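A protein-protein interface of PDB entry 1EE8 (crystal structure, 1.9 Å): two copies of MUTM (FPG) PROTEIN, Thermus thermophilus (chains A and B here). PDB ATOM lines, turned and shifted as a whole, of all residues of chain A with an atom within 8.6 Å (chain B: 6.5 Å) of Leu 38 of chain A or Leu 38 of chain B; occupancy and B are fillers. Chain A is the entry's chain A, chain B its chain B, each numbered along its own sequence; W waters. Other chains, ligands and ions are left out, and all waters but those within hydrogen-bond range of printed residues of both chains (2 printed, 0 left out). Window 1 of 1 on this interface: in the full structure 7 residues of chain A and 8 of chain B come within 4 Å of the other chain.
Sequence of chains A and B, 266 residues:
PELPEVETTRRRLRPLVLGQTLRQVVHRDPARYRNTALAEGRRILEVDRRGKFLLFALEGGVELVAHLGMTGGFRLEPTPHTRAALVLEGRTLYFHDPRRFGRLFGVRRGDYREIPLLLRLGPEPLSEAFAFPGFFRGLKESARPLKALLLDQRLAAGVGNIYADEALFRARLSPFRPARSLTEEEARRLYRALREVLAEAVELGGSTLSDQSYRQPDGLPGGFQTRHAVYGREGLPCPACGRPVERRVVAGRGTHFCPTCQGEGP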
ATOM      1  N   LEU A  22      19.749 -23.078  37.398  1.00  0.00           N
ATOM      2  CA  LEU A  22      19.323 -23.840  36.231  1.00  0.00           C
ATOM      3  C   LEU A  22      20.467 -24.828  36.001  1.00  0.00           C
ATOM      4  O   LEU A  22      21.486 -24.483  35.392  1.00  0.00           O
ATOM      5  CB  LEU A  22      19.145 -22.925  35.018  1.00  0.00           C
ATOM      6  CG  LEU A  22      18.949 -23.637  33.673  1.00  0.00           C
ATOM      7  CD1 LEU A  22      17.663 -24.462  33.690  1.00  0.00           C
ATOM      8  CD2 LEU A  22      18.907 -22.603  32.552  1.00  0.00           C
ATOM      9  N   VAL A  25      19.533 -27.961  30.726  1.00  0.00           N
ATOM     10  CA  VAL A  25      18.465 -27.797  29.759  1.00  0.00           C
ATOM     11  C   VAL A  25      18.575 -29.083  28.973  1.00  0.00           C
ATOM     12  O   VAL A  25      19.493 -29.265  28.167  1.00  0.00           O
ATOM     13  CB  VAL A  25      18.700 -26.607  28.812  1.00  0.00           C
ATOM     14  CG1 VAL A  25      17.490 -26.435  27.896  1.00  0.00           C
ATOM     15  CG2 VAL A  25      18.940 -25.343  29.618  1.00  0.00           C
ATOM     16  N   ARG A  34      18.923 -24.082  20.398  1.00  0.00           N
ATOM     17  CA  ARG A  34      20.307 -23.741  20.111  1.00  0.00           C
ATOM     18  C   ARG A  34      21.134 -23.149  21.230  1.00  0.00           C
ATOM     19  O   ARG A  34      20.687 -22.243  21.941  1.00  0.00           O
ATOM     20  CB  ARG A  34      20.335 -22.788  18.923  1.00  0.00           C
ATOM     21  CG  ARG A  34      19.614 -23.326  17.706  1.00  0.00           C
ATOM     22  CD  ARG A  34      19.330 -22.222  16.696  1.00  0.00           C
ATOM     23  NE  ARG A  34      18.446 -22.703  15.639  1.00  0.00           N
ATOM     24  CZ  ARG A  34      17.674 -21.922  14.888  1.00  0.00           C
ATOM     25  NH1 ARG A  34      17.671 -20.607  15.073  1.00  0.00           N
ATOM     26  NH2 ARG A  34      16.905 -22.459  13.949  1.00  0.00           N
ATOM     27  N   ASN A  35      22.353 -23.668  21.365  1.00  0.00           N
ATOM     28  CA  ASN A  35      23.300 -23.192  22.363  1.00  0.00           C
ATOM     29  C   ASN A  35      22.729 -23.143  23.769  1.00  0.00           C
ATOM     30  O   ASN A  35      23.018 -22.219  24.522  1.00  0.00           O
ATOM     31  CB  ASN A  35      23.794 -21.794  21.970  1.00  0.00           C
ATOM     32  CG  ASN A  35      24.431 -21.772  20.595  1.00  0.00           C
ATOM     33  OD1 ASN A  35      23.958 -21.091  19.680  1.00  0.00           O
ATOM     34  ND2 ASN A  35      25.507 -22.525  20.440  1.00  0.00           N
ATOM     35  N   THR A  36      21.926 -24.133  24.136  1.00  0.00           N
ATOM     36  CA  THR A  36      21.346 -24.138  25.475  1.00  0.00           C
ATOM     37  C   THR A  36      22.382 -24.450  26.562  1.00  0.00           C
ATOM     38  O   THR A  36      22.194 -24.076  27.715  1.00  0.00           O
ATOM     39  CB  THR A  36      20.175 -25.140  25.575  1.00  0.00           C
ATOM     40  OG1 THR A  36      20.634 -26.454  25.233  1.00  0.00           O
ATOM     41  CG2 THR A  36      19.060 -24.738  24.627  1.00  0.00           C
ATOM     42  N   ALA A  37      23.479 -25.111  26.197  1.00  0.00           N
ATOM     43  CA  ALA A  37      24.519 -25.447  27.178  1.00  0.00           C
ATOM     44  C   ALA A  37      25.081 -24.174  27.813  1.00  0.00           C
ATOM     45  O   ALA A  37      25.604 -24.191  28.925  1.00  0.00           O
ATOM     46  CB  ALA A  37      25.643 -26.236  26.514  1.00  0.00           C
ATOM     47  N   LEU A  38      24.953 -23.067  27.096  1.00  0.00           N
ATOM     48  CA  LEU A  38      25.443 -21.787  27.575  1.00  0.00           C
ATOM     49  C   LEU A  38      24.755 -21.385  28.873  1.00  0.00           C
ATOM     50  O   LEU A  38      25.353 -20.748  29.744  1.00  0.00           O
ATOM     51  CB  LEU A  38      25.184 -20.724  26.511  1.00  0.00           C
ATOM     52  CG  LEU A  38      26.265 -19.676  26.291  1.00  0.00           C
ATOM     53  CD1 LEU A  38      27.535 -20.365  25.843  1.00  0.00           C
ATOM     54  CD2 LEU A  38      25.797 -18.675  25.250  1.00  0.00           C
ATOM     55  N   ALA A  39      23.492 -21.769  28.994  1.00  0.00           N
ATOM     56  CA  ALA A  39      22.674 -21.435  30.154  1.00  0.00           C
ATOM     57  C   ALA A  39      22.847 -22.345  31.362  1.00  0.00           C
ATOM     58  O   ALA A  39      22.479 -21.974  32.476  1.00  0.00           O
ATOM     59  CB  ALA A  39      21.198 -21.428  29.743  1.00  0.00           C
ATOM     60  N   GLU A  40      23.405 -23.529  31.149  1.00  0.00           N
ATOM     61  CA  GLU A  40      23.559 -24.496  32.227  1.00  0.00           C
ATOM     62  C   GLU A  40      24.514 -24.130  33.361  1.00  0.00           C
ATOM     63  O   GLU A  40      25.596 -23.572  33.146  1.00  0.00           O
ATOM     64  CB  GLU A  40      23.932 -25.858  31.638  1.00  0.00           C
ATOM     65  CG  GLU A  40      22.838 -26.423  30.740  1.00  0.00           C
ATOM     66  CD  GLU A  40      23.178 -27.795  30.188  1.00  0.00           C
ATOM     67  OE1 GLU A  40      22.246 -28.597  29.980  1.00  0.00           O
ATOM     68  OE2 GLU A  40      24.372 -28.070  29.955  1.00  0.00           O
ATOM     69  N   GLY A  41      24.079 -24.444  34.578  1.00  0.00           N
ATOM     70  CA  GLY A  41      24.866 -24.173  35.761  1.00  0.00           C
ATOM     71  C   GLY A  41      24.885 -22.711  36.149  1.00  0.00           C
ATOM     72  O   GLY A  41      25.897 -22.213  36.616  1.00  0.00           O
ATOM     73  N   ARG A  42      23.767 -22.023  35.953  1.00  0.00           N
ATOM     74  CA  ARG A  42      23.683 -20.608  36.285  1.00  0.00           C
ATOM     75  C   ARG A  42      22.385 -20.352  37.031  1.00  0.00           C
ATOM     76  O   ARG A  42      21.366 -21.006  36.773  1.00  0.00           O
ATOM     77  CB  ARG A  42      23.702 -19.756  35.010  1.00  0.00           C
ATOM     78  CG  ARG A  42      24.941 -19.910  34.150  1.00  0.00           C
ATOM     79  CD  ARG A  42      24.782 -19.119  32.873  1.00  0.00           C
ATOM     80  NE  ARG A  42      25.887 -19.333  31.940  1.00  0.00           N
ATOM     81  CZ  ARG A  42      27.080 -18.748  32.024  1.00  0.00           C
ATOM     82  NH1 ARG A  42      27.356 -17.897  32.997  1.00  0.00           N
ATOM     83  NH2 ARG A  42      27.999 -19.017  31.117  1.00  0.00           N
ATOM     84  N   LEU A  58      20.229 -15.095  33.272  1.00  0.00           N
ATOM     85  CA  LEU A  58      21.077 -15.979  34.053  1.00  0.00           C
ATOM     86  C   LEU A  58      22.370 -15.319  34.512  1.00  0.00           C
ATOM     87  O   LEU A  58      23.003 -14.566  33.771  1.00  0.00           O
ATOM     88  CB  LEU A  58      21.391 -17.221  33.223  1.00  0.00           C
ATOM     89  CG  LEU A  58      20.122 -17.859  32.652  1.00  0.00           C
ATOM     90  CD1 LEU A  58      20.484 -18.914  31.625  1.00  0.00           C
ATOM     91  CD2 LEU A  58      19.297 -18.454  33.793  1.00  0.00           C
ATOM     92  N   GLU A  59      22.760 -15.619  35.741  1.00  0.00           N
ATOM     93  CA  GLU A  59      23.973 -15.066  36.319  1.00  0.00           C
ATOM     94  C   GLU A  59      25.163 -15.315  35.395  1.00  0.00           C
ATOM     95  O   GLU A  59      25.347 -16.421  34.892  1.00  0.00           O
ATOM     96  CB  GLU A  59      24.205 -15.715  37.677  1.00  0.00           C
ATOM     97  CG  GLU A  59      25.285 -15.072  38.517  1.00  0.00           C
ATOM     98  CD  GLU A  59      25.270 -15.603  39.936  1.00  0.00           C
ATOM     99  OE1 GLU A  59      25.375 -16.837  40.111  1.00  0.00           O
ATOM    100  OE2 GLU A  59      25.149 -14.787  40.874  1.00  0.00           O
ATOM    101  N   GLY A  60      25.967 -14.281  35.157  1.00  0.00           N
ATOM    102  CA  GLY A  60      27.119 -14.448  34.292  1.00  0.00           C
ATOM    103  C   GLY A  60      26.945 -13.857  32.906  1.00  0.00           C
ATOM    104  O   GLY A  60      27.739 -14.130  32.004  1.00  0.00           O
ATOM    105  N   GLY A  61      25.896 -13.059  32.731  1.00  0.00           N
ATOM    106  CA  GLY A  61      25.655 -12.409  31.453  1.00  0.00           C
ATOM    107  C   GLY A  61      25.128 -13.278  30.329  1.00  0.00           C
ATOM    108  O   GLY A  61      25.519 -13.110  29.177  1.00  0.00           O
ATOM    109  N   VAL A  62      24.236 -14.202  30.661  1.00  0.00           N
ATOM    110  CA  VAL A  62      23.649 -15.094  29.672  1.00  0.00           C
ATOM    111  C   VAL A  62      22.125 -14.997  29.705  1.00  0.00           C
ATOM    112  O   VAL A  62      21.538 -14.663  30.735  1.00  0.00           O
ATOM    113  CB  VAL A  62      24.051 -16.567  29.953  1.00  0.00           C
ATOM    114  CG1 VAL A  62      23.138 -17.513  29.194  1.00  0.00           C
ATOM    115  CG2 VAL A  62      25.514 -16.801  29.549  1.00  0.00           C
ATOM    116  N   GLU A  63      21.490 -15.276  28.572  1.00  0.00           N
ATOM    117  CA  GLU A  63      20.037 -15.272  28.503  1.00  0.00           C
ATOM    118  C   GLU A  63      19.547 -16.502  27.754  1.00  0.00           C
ATOM    119  O   GLU A  63      20.127 -16.907  26.746  1.00  0.00           O
ATOM    120  CB  GLU A  63      19.506 -14.018  27.789  1.00  0.00           C
ATOM    121  CG  GLU A  63      19.838 -12.704  28.476  1.00  0.00           C
ATOM    122  CD  GLU A  63      19.228 -11.496  27.777  1.00  0.00           C
ATOM    123  OE1 GLU A  63      19.516 -11.272  26.578  1.00  0.00           O
ATOM    124  OE2 GLU A  63      18.462 -10.762  28.433  1.00  0.00           O
ATOM    125  N   LEU A  64      18.488 -17.114  28.266  1.00  0.00           N
ATOM    126  CA  LEU A  64      17.901 -18.251  27.589  1.00  0.00           C
ATOM    127  C   LEU A  64      16.605 -17.668  27.048  1.00  0.00           C
ATOM    128  O   LEU A  64      15.674 -17.382  27.799  1.00  0.00           O
ATOM    129  CB  LEU A  64      17.619 -19.397  28.558  1.00  0.00           C
ATOM    130  CG  LEU A  64      17.073 -20.678  27.918  1.00  0.00           C
ATOM    131  CD1 LEU A  64      18.030 -21.185  26.845  1.00  0.00           C
ATOM    132  CD2 LEU A  64      16.881 -21.734  28.994  1.00  0.00           C
ATOM    133  N   PHE A 105      16.891 -20.253  22.611  1.00  0.00           N
ATOM    134  CA  PHE A 105      18.148 -19.640  22.208  1.00  0.00           C
ATOM    135  C   PHE A 105      19.027 -19.309  23.402  1.00  0.00           C
ATOM    136  O   PHE A 105      18.645 -18.519  24.268  1.00  0.00           O
ATOM    137  CB  PHE A 105      17.887 -18.337  21.449  1.00  0.00           C
ATOM    138  CG  PHE A 105      17.006 -18.489  20.249  1.00  0.00           C
ATOM    139  CD1 PHE A 105      17.548 -18.791  19.003  1.00  0.00           C
ATOM    140  CD2 PHE A 105      15.632 -18.301  20.356  1.00  0.00           C
ATOM    141  CE1 PHE A 105      16.732 -18.900  17.876  1.00  0.00           C
ATOM    142  CE2 PHE A 105      14.806 -18.409  19.230  1.00  0.00           C
ATOM    143  CZ  PHE A 105      15.364 -18.707  17.989  1.00  0.00           C
ATOM    144  N   GLY A 106      20.204 -19.917  23.446  1.00  0.00           N
ATOM    145  CA  GLY A 106      21.140 -19.620  24.512  1.00  0.00           C
ATOM    146  C   GLY A 106      21.993 -18.517  23.918  1.00  0.00           C
ATOM    147  O   GLY A 106      22.577 -18.695  22.849  1.00  0.00           O
ATOM    148  N   VAL A 107      22.058 -17.372  24.579  1.00  0.00           N
ATOM    149  CA  VAL A 107      22.845 -16.267  24.040  1.00  0.00           C
ATOM    150  C   VAL A 107      23.503 -15.417  25.117  1.00  0.00           C
ATOM    151  O   VAL A 107      23.030 -15.367  26.246  1.00  0.00           O
ATOM    152  CB  VAL A 107      21.966 -15.313  23.203  1.00  0.00           C
ATOM    153  CG1 VAL A 107      21.361 -16.047  22.003  1.00  0.00           C
ATOM    154  CG2 VAL A 107      20.877 -14.729  24.084  1.00  0.00           C
ATOM    155  N   ARG A 108      24.605 -14.763  24.764  1.00  0.00           N
ATOM    156  CA  ARG A 108      25.256 -13.863  25.703  1.00  0.00           C
ATOM    157  C   ARG A 108      24.194 -12.773  25.822  1.00  0.00           C
ATOM    158  O   ARG A 108      23.489 -12.501  24.853  1.00  0.00           O
ATOM    159  CB  ARG A 108      26.534 -13.286  25.100  1.00  0.00           C
ATOM    160  CG  ARG A 108      27.640 -14.309  24.904  1.00  0.00           C
ATOM    161  CD  ARG A 108      28.797 -14.059  25.870  1.00  0.00           C
ATOM    162  NE  ARG A 108      28.384 -14.098  27.273  1.00  0.00           N
ATOM    163  CZ  ARG A 108      29.193 -13.833  28.297  1.00  0.00           C
ATOM    164  NH1 ARG A 108      30.463 -13.507  28.075  1.00  0.00           N
ATOM    165  NH2 ARG A 108      28.737 -13.892  29.542  1.00  0.00           N
ATOM    166  N   ARG A 109      24.070 -12.165  26.992  1.00  0.00           N
ATOM    167  CA  ARG A 109      23.060 -11.132  27.212  1.00  0.00           C
ATOM    168  C   ARG A 109      23.091 -10.024  26.157  1.00  0.00           C
ATOM    169  O   ARG A 109      24.119  -9.374  25.951  1.00  0.00           O
ATOM    170  CB  ARG A 109      23.240 -10.528  28.602  1.00  0.00           C
ATOM    171  CG  ARG A 109      22.175  -9.528  29.014  1.00  0.00           C
ATOM    172  CD  ARG A 109      22.449  -9.017  30.424  1.00  0.00           C
ATOM    173  NE  ARG A 109      21.321  -8.267  30.975  1.00  0.00           N
ATOM    174  CZ  ARG A 109      20.150  -8.806  31.313  1.00  0.00           C
ATOM    175  NH1 ARG A 109      19.941 -10.109  31.163  1.00  0.00           N
ATOM    176  NH2 ARG A 109      19.179  -8.037  31.795  1.00  0.00           N
ATOM    177  N   ASP A 111      22.923 -10.303  22.888  1.00  0.00           N
ATOM    178  CA  ASP A 111      23.296 -10.774  21.553  1.00  0.00           C
ATOM    179  C   ASP A 111      22.125 -11.439  20.843  1.00  0.00           C
ATOM    180  O   ASP A 111      21.955 -12.658  20.893  1.00  0.00           O
ATOM    181  CB  ASP A 111      24.483 -11.740  21.640  1.00  0.00           C
ATOM    182  CG  ASP A 111      24.877 -12.311  20.284  1.00  0.00           C
ATOM    183  OD1 ASP A 111      24.696 -11.615  19.260  1.00  0.00           O
ATOM    184  OD2 ASP A 111      25.383 -13.455  20.242  1.00  0.00           O
ATOM    185  N   GLU A 114      20.817 -13.664  16.324  1.00  0.00           N
ATOM    186  CA  GLU A 114      20.093 -14.842  15.864  1.00  0.00           C
ATOM    187  C   GLU A 114      18.591 -14.656  16.024  1.00  0.00           C
ATOM    188  O   GLU A 114      17.802 -15.405  15.452  1.00  0.00           O
ATOM    189  CB  GLU A 114      20.543 -16.074  16.648  1.00  0.00           C
ATOM    190  CG  GLU A 114      21.935 -16.569  16.283  1.00  0.00           C
ATOM    191  CD  GLU A 114      22.474 -17.588  17.270  1.00  0.00           C
ATOM    192  OE1 GLU A 114      23.450 -18.286  16.924  1.00  0.00           O
ATOM    193  OE2 GLU A 114      21.932 -17.683  18.396  1.00  0.00           O
ATOM    194  N   ASN B  35      33.626 -23.214  21.253  1.00  0.00           N
ATOM    195  CA  ASN B  35      32.596 -23.017  22.272  1.00  0.00           C
ATOM    196  C   ASN B  35      33.092 -22.343  23.537  1.00  0.00           C
ATOM    197  O   ASN B  35      32.677 -22.701  24.640  1.00  0.00           O
ATOM    198  CB  ASN B  35      31.969 -24.363  22.641  1.00  0.00           C
ATOM    199  CG  ASN B  35      31.390 -25.071  21.448  1.00  0.00           C
ATOM    200  OD1 ASN B  35      30.511 -24.545  20.770  1.00  0.00           O
ATOM    201  ND2 ASN B  35      31.879 -26.273  21.178  1.00  0.00           N
ATOM    202  N   THR B  36      33.963 -21.356  23.391  1.00  0.00           N
ATOM    203  CA  THR B  36      34.488 -20.686  24.567  1.00  0.00           C
ATOM    204  C   THR B  36      33.421 -19.883  25.310  1.00  0.00           C
ATOM    205  O   THR B  36      33.552 -19.651  26.506  1.00  0.00           O
ATOM    206  CB  THR B  36      35.666 -19.769  24.197  1.00  0.00           C
ATOM    207  OG1 THR B  36      35.230 -18.801  23.241  1.00  0.00           O
ATOM    208  CG2 THR B  36      36.813 -20.589  23.597  1.00  0.00           C
ATOM    209  N   ALA B  37      32.361 -19.477  24.612  1.00  0.00           N
ATOM    210  CA  ALA B  37      31.297 -18.695  25.243  1.00  0.00           C
ATOM    211  C   ALA B  37      30.708 -19.458  26.416  1.00  0.00           C
ATOM    212  O   ALA B  37      30.178 -18.870  27.360  1.00  0.00           O
ATOM    213  CB  ALA B  37      30.194 -18.370  24.229  1.00  0.00           C
ATOM    214  N   LEU B  38      30.820 -20.778  26.357  1.00  0.00           N
ATOM    215  CA  LEU B  38      30.289 -21.622  27.405  1.00  0.00           C
ATOM    216  C   LEU B  38      30.990 -21.361  28.739  1.00  0.00           C
ATOM    217  O   LEU B  38      30.388 -21.462  29.803  1.00  0.00           O
ATOM    218  CB  LEU B  38      30.456 -23.090  26.990  1.00  0.00           C
ATOM    219  CG  LEU B  38      30.005 -24.145  27.997  1.00  0.00           C
ATOM    220  CD1 LEU B  38      28.561 -23.902  28.404  1.00  0.00           C
ATOM    221  CD2 LEU B  38      30.167 -25.523  27.368  1.00  0.00           C
ATOM    222  N   ALA B  39      32.266 -21.010  28.671  1.00  0.00           N
ATOM    223  CA  ALA B  39      33.063 -20.770  29.870  1.00  0.00           C
ATOM    224  C   ALA B  39      32.920 -19.382  30.478  1.00  0.00           C
ATOM    225  O   ALA B  39      33.274 -19.179  31.638  1.00  0.00           O
ATOM    226  CB  ALA B  39      34.537 -21.030  29.559  1.00  0.00           C
ATOM    227  N   GLU B  40      32.392 -18.434  29.711  1.00  0.00           N
ATOM    228  CA  GLU B  40      32.284 -17.063  30.184  1.00  0.00           C
ATOM    229  C   GLU B  40      31.271 -16.818  31.291  1.00  0.00           C
ATOM    230  O   GLU B  40      30.212 -17.453  31.347  1.00  0.00           O
ATOM    231  CB  GLU B  40      32.020 -16.121  29.000  1.00  0.00           C
ATOM    232  CG  GLU B  40      33.160 -16.118  27.967  1.00  0.00           C
ATOM    233  CD  GLU B  40      32.900 -15.193  26.776  1.00  0.00           C
ATOM    234  OE1 GLU B  40      33.841 -14.480  26.343  1.00  0.00           O
ATOM    235  OE2 GLU B  40      31.760 -15.184  26.266  1.00  0.00           O
ATOM    236  N   GLY B  41      31.621 -15.886  32.174  1.00  0.00           N
ATOM    237  CA  GLY B  41      30.763 -15.541  33.288  1.00  0.00           C
ATOM    238  C   GLY B  41      30.712 -16.614  34.357  1.00  0.00           C
ATOM    239  O   GLY B  41      29.685 -16.774  35.012  1.00  0.00           O
ATOM    240  N   ARG B  42      31.815 -17.342  34.541  1.00  0.00           N
ATOM    241  CA  ARG B  42      31.885 -18.412  35.542  1.00  0.00           C
ATOM    242  C   ARG B  42      33.137 -18.282  36.410  1.00  0.00           C
ATOM    243  O   ARG B  42      34.212 -17.908  35.935  1.00  0.00           O
ATOM    244  CB  ARG B  42      31.902 -19.786  34.855  1.00  0.00           C
ATOM    245  CG  ARG B  42      30.640 -20.125  34.040  1.00  0.00           C
ATOM    246  CD  ARG B  42      30.805 -21.477  33.331  1.00  0.00           C
ATOM    247  NE  ARG B  42      29.736 -21.768  32.371  1.00  0.00           N
ATOM    248  CZ  ARG B  42      28.494 -22.119  32.690  1.00  0.00           C
ATOM    249  NH1 ARG B  42      28.132 -22.233  33.963  1.00  0.00           N
ATOM    250  NH2 ARG B  42      27.603 -22.359  31.728  1.00  0.00           N
ATOM    251  N   LEU B  58      35.222 -24.835  35.955  1.00  0.00           N
ATOM    252  CA  LEU B  58      34.400 -23.646  36.120  1.00  0.00           C
ATOM    253  C   LEU B  58      33.096 -23.937  36.832  1.00  0.00           C
ATOM    254  O   LEU B  58      32.515 -25.019  36.686  1.00  0.00           O
ATOM    255  CB  LEU B  58      34.121 -23.019  34.750  1.00  0.00           C
ATOM    256  CG  LEU B  58      35.402 -22.647  33.987  1.00  0.00           C
ATOM    257  CD1 LEU B  58      35.085 -22.297  32.545  1.00  0.00           C
ATOM    258  CD2 LEU B  58      36.079 -21.473  34.699  1.00  0.00           C
ATOM    259  N   VAL B  62      31.260 -26.828  34.141  1.00  0.00           N
ATOM    260  CA  VAL B  62      31.887 -26.612  32.837  1.00  0.00           C
ATOM    261  C   VAL B  62      33.405 -26.593  32.974  1.00  0.00           C
ATOM    262  O   VAL B  62      33.938 -26.297  34.043  1.00  0.00           O
ATOM    263  CB  VAL B  62      31.392 -25.264  32.220  1.00  0.00           C
ATOM    264  CG1 VAL B  62      32.212 -24.881  30.994  1.00  0.00           C
ATOM    265  CG2 VAL B  62      29.916 -25.395  31.836  1.00  0.00           C
ATOM    266  N   GLU B  63      34.098 -26.945  31.899  1.00  0.00           N
ATOM    267  CA  GLU B  63      35.552 -26.922  31.893  1.00  0.00           C
ATOM    268  C   GLU B  63      36.029 -26.213  30.632  1.00  0.00           C
ATOM    269  O   GLU B  63      35.395 -26.295  29.576  1.00  0.00           O
ATOM    270  CB  GLU B  63      36.148 -28.338  31.906  1.00  0.00           C
ATOM    271  CG  GLU B  63      35.960 -29.125  33.190  1.00  0.00           C
ATOM    272  CD  GLU B  63      36.590 -30.512  33.108  1.00  0.00           C
ATOM    273  OE1 GLU B  63      36.305 -31.244  32.136  1.00  0.00           O
ATOM    274  OE2 GLU B  63      37.371 -30.872  34.016  1.00  0.00           O
ATOM    275  N   GLY B 106      35.459 -25.209  25.183  1.00  0.00           N
ATOM    276  CA  GLY B 106      34.528 -24.991  26.270  1.00  0.00           C
ATOM    277  C   GLY B 106      33.659 -26.230  26.259  1.00  0.00           C
ATOM    278  O   GLY B 106      32.997 -26.519  25.256  1.00  0.00           O
ATOM    279  N   VAL B 107      33.671 -26.986  27.349  1.00  0.00           N
ATOM    280  CA  VAL B 107      32.879 -28.211  27.404  1.00  0.00           C
ATOM    281  C   VAL B 107      32.195 -28.444  28.738  1.00  0.00           C
ATOM    282  O   VAL B 107      32.545 -27.836  29.750  1.00  0.00           O
ATOM    283  CB  VAL B 107      33.759 -29.456  27.113  1.00  0.00           C
ATOM    284  CG1 VAL B 107      34.425 -29.325  25.749  1.00  0.00           C
ATOM    285  CG2 VAL B 107      34.829 -29.615  28.189  1.00  0.00           C
ATOM    286  N   ARG B 108      31.200 -29.328  28.730  1.00  0.00           N
ATOM    287  CA  ARG B 108      30.522 -29.688  29.965  1.00  0.00           C
ATOM    288  C   ARG B 108      31.571 -30.571  30.653  1.00  0.00           C
ATOM    289  O   ARG B 108      32.306 -31.300  29.985  1.00  0.00           O
ATOM    290  CB  ARG B 108      29.242 -30.475  29.654  1.00  0.00           C
ATOM    291  CG  ARG B 108      28.173 -30.370  30.726  1.00  0.00           C
ATOM    292  CD  ARG B 108      26.816 -30.832  30.205  1.00  0.00           C
ATOM    293  NE  ARG B 108      26.348 -30.004  29.094  1.00  0.00           N
ATOM    294  CZ  ARG B 108      25.212 -30.206  28.430  1.00  0.00           C
ATOM    295  NH1 ARG B 108      24.868 -29.401  27.431  1.00  0.00           N
ATOM    296  NH2 ARG B 108      24.416 -31.212  28.764  1.00  0.00           N
HETATM  297  O   HOH W   1      22.529 -31.255  30.546  1.00  0.00           O
HETATM  298  O   HOH W   2      28.538 -17.700  29.036  1.00  0.00           O
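Water W2 lies within hydrogen-bond range of the guanidinium group (NH2) of Arg 42 of chain A, the backbone carbonyl oxygen (O) of Ala 37 of chain B and the backbone carbonyl oxygen (O) of Glu 40 of chain B.
The guanidinium group (NH1) of Arg 42 of chain A sits at hydrogen-bond distance from the backbone carbonyl oxygen (O) of Glu 59 of chain A. The backbone carbonyl oxygen of Leu 38 of chain A lies within hydrogen-bond range of the guanidinium group of Arg 42 of chain A (2.7 Å).
The backbone carbonyl oxygen (O) of Leu 38 of chain A lies within hydrogen-bond range of the guanidinium group (NH2) of Arg 42 of chain B (3.4 Å). The guanidinium group of Arg 42 of chain B is in hydrogen-bond range of the backbone carbonyl oxygen of Glu 40 of chain A, 2.7 Å away. The backbone carbonyl oxygen (O) of Gly 41 of chain A sits at hydrogen-bond distance from the guanidinium group (NH1) of Arg 42 of chain B (3.5 Å). O of Gly 41 of chain B lies within hydrogen-bond range of NH1 of Arg 42 of chain A, at 3.3 Å. The backbone carbonyl oxygen (O) of Glu 40 of chain B sits at hydrogen-bond distance from the guanidinium group (NH2) of Arg 42 of chain A (2.7 Å). The guanidinium group of Arg 108 of chain A lies within salt-bridge range of the side-chain carboxylate of Glu 40 of chain B, 2.8 Å away. The side-chain carboxylate (OE2) of Glu 40 of chain A lies within salt-bridge range of the guanidinium group (NE) of Arg 108 of chain B. The guanidinium group (NH2) of Arg 42 of chain A sits close to the guanidinium group (NH2) of Arg 42 of chain B.
Glu 40 of chain A touches Arg 42 of chain B, and with the chains exchanged Arg 42 of chain A touches Glu 40 of chain B. Gly 41 of chain A touches Arg 42 of chain B, and with the chains exchanged Arg 42 of chain A touches Gly 41 of chain B. Positions printed for both chains: 35, 36, 37, 38, 39, 40, 41, 42, 58, 62, 63, 106, 107 and 108.
Leu 38 of chain A touches just these residues of chain B: Ala 37, Leu 38 and Arg 42. Leu 38 of chain B touches three residues of chain A. Ala 37 of chain B touches just one residue of chain A: Leu 38 (3.3 Å). No residue of chain A comes within 4 Å of Ala 39 of chain B. Of the printed residues of chain B, Glu 40 of chain A touches Arg 42 (2.7 Å) and Arg 108 (2.8 Å). Printed residues of chain A within 4 Å of Arg 42 of chain B: Ala 37, Leu 38, Glu 40, Gly 41 and Arg 42. Of the printed residues of chain A, Gly 41 of chain B touches Arg 42 (3.3 Å) and Gly 60 (3.5 Å). The nearest residue of chain B that does not touch Leu 38 of chain A is Ala 39 of chain B (5.5 Å).
Among the printed residues, merely in contact across the chains: Ala 37 of chain A with Leu 38 of chain B (3.0 Å), Ala 37 of chain A with Arg 42 of chain B (3.9 Å), Ala 37 of chain A with Arg 108 of chain B (3.4 Å), Leu 38 of chain A with Ala 37 of chain B (3.3 Å), Leu 38 of chain A with Leu 38 of chain B (3.4 Å), Arg 42 of chain A with Leu 38 of chain B (3.7 Å) and Gly 60 of chain A with Gly 41 of chain B (3.5 Å).
Of the 14 printed residues of chain B, 6 touch a printed residue of chain A. Hydrophobic or aromatic side chains of chain B that line the printed part of chain A: Ala 37 and Leu 38. Hydrophobic or aromatic side chains of chain A within 4 Å of the printed part of chain B: Ala 37 and Leu 38.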
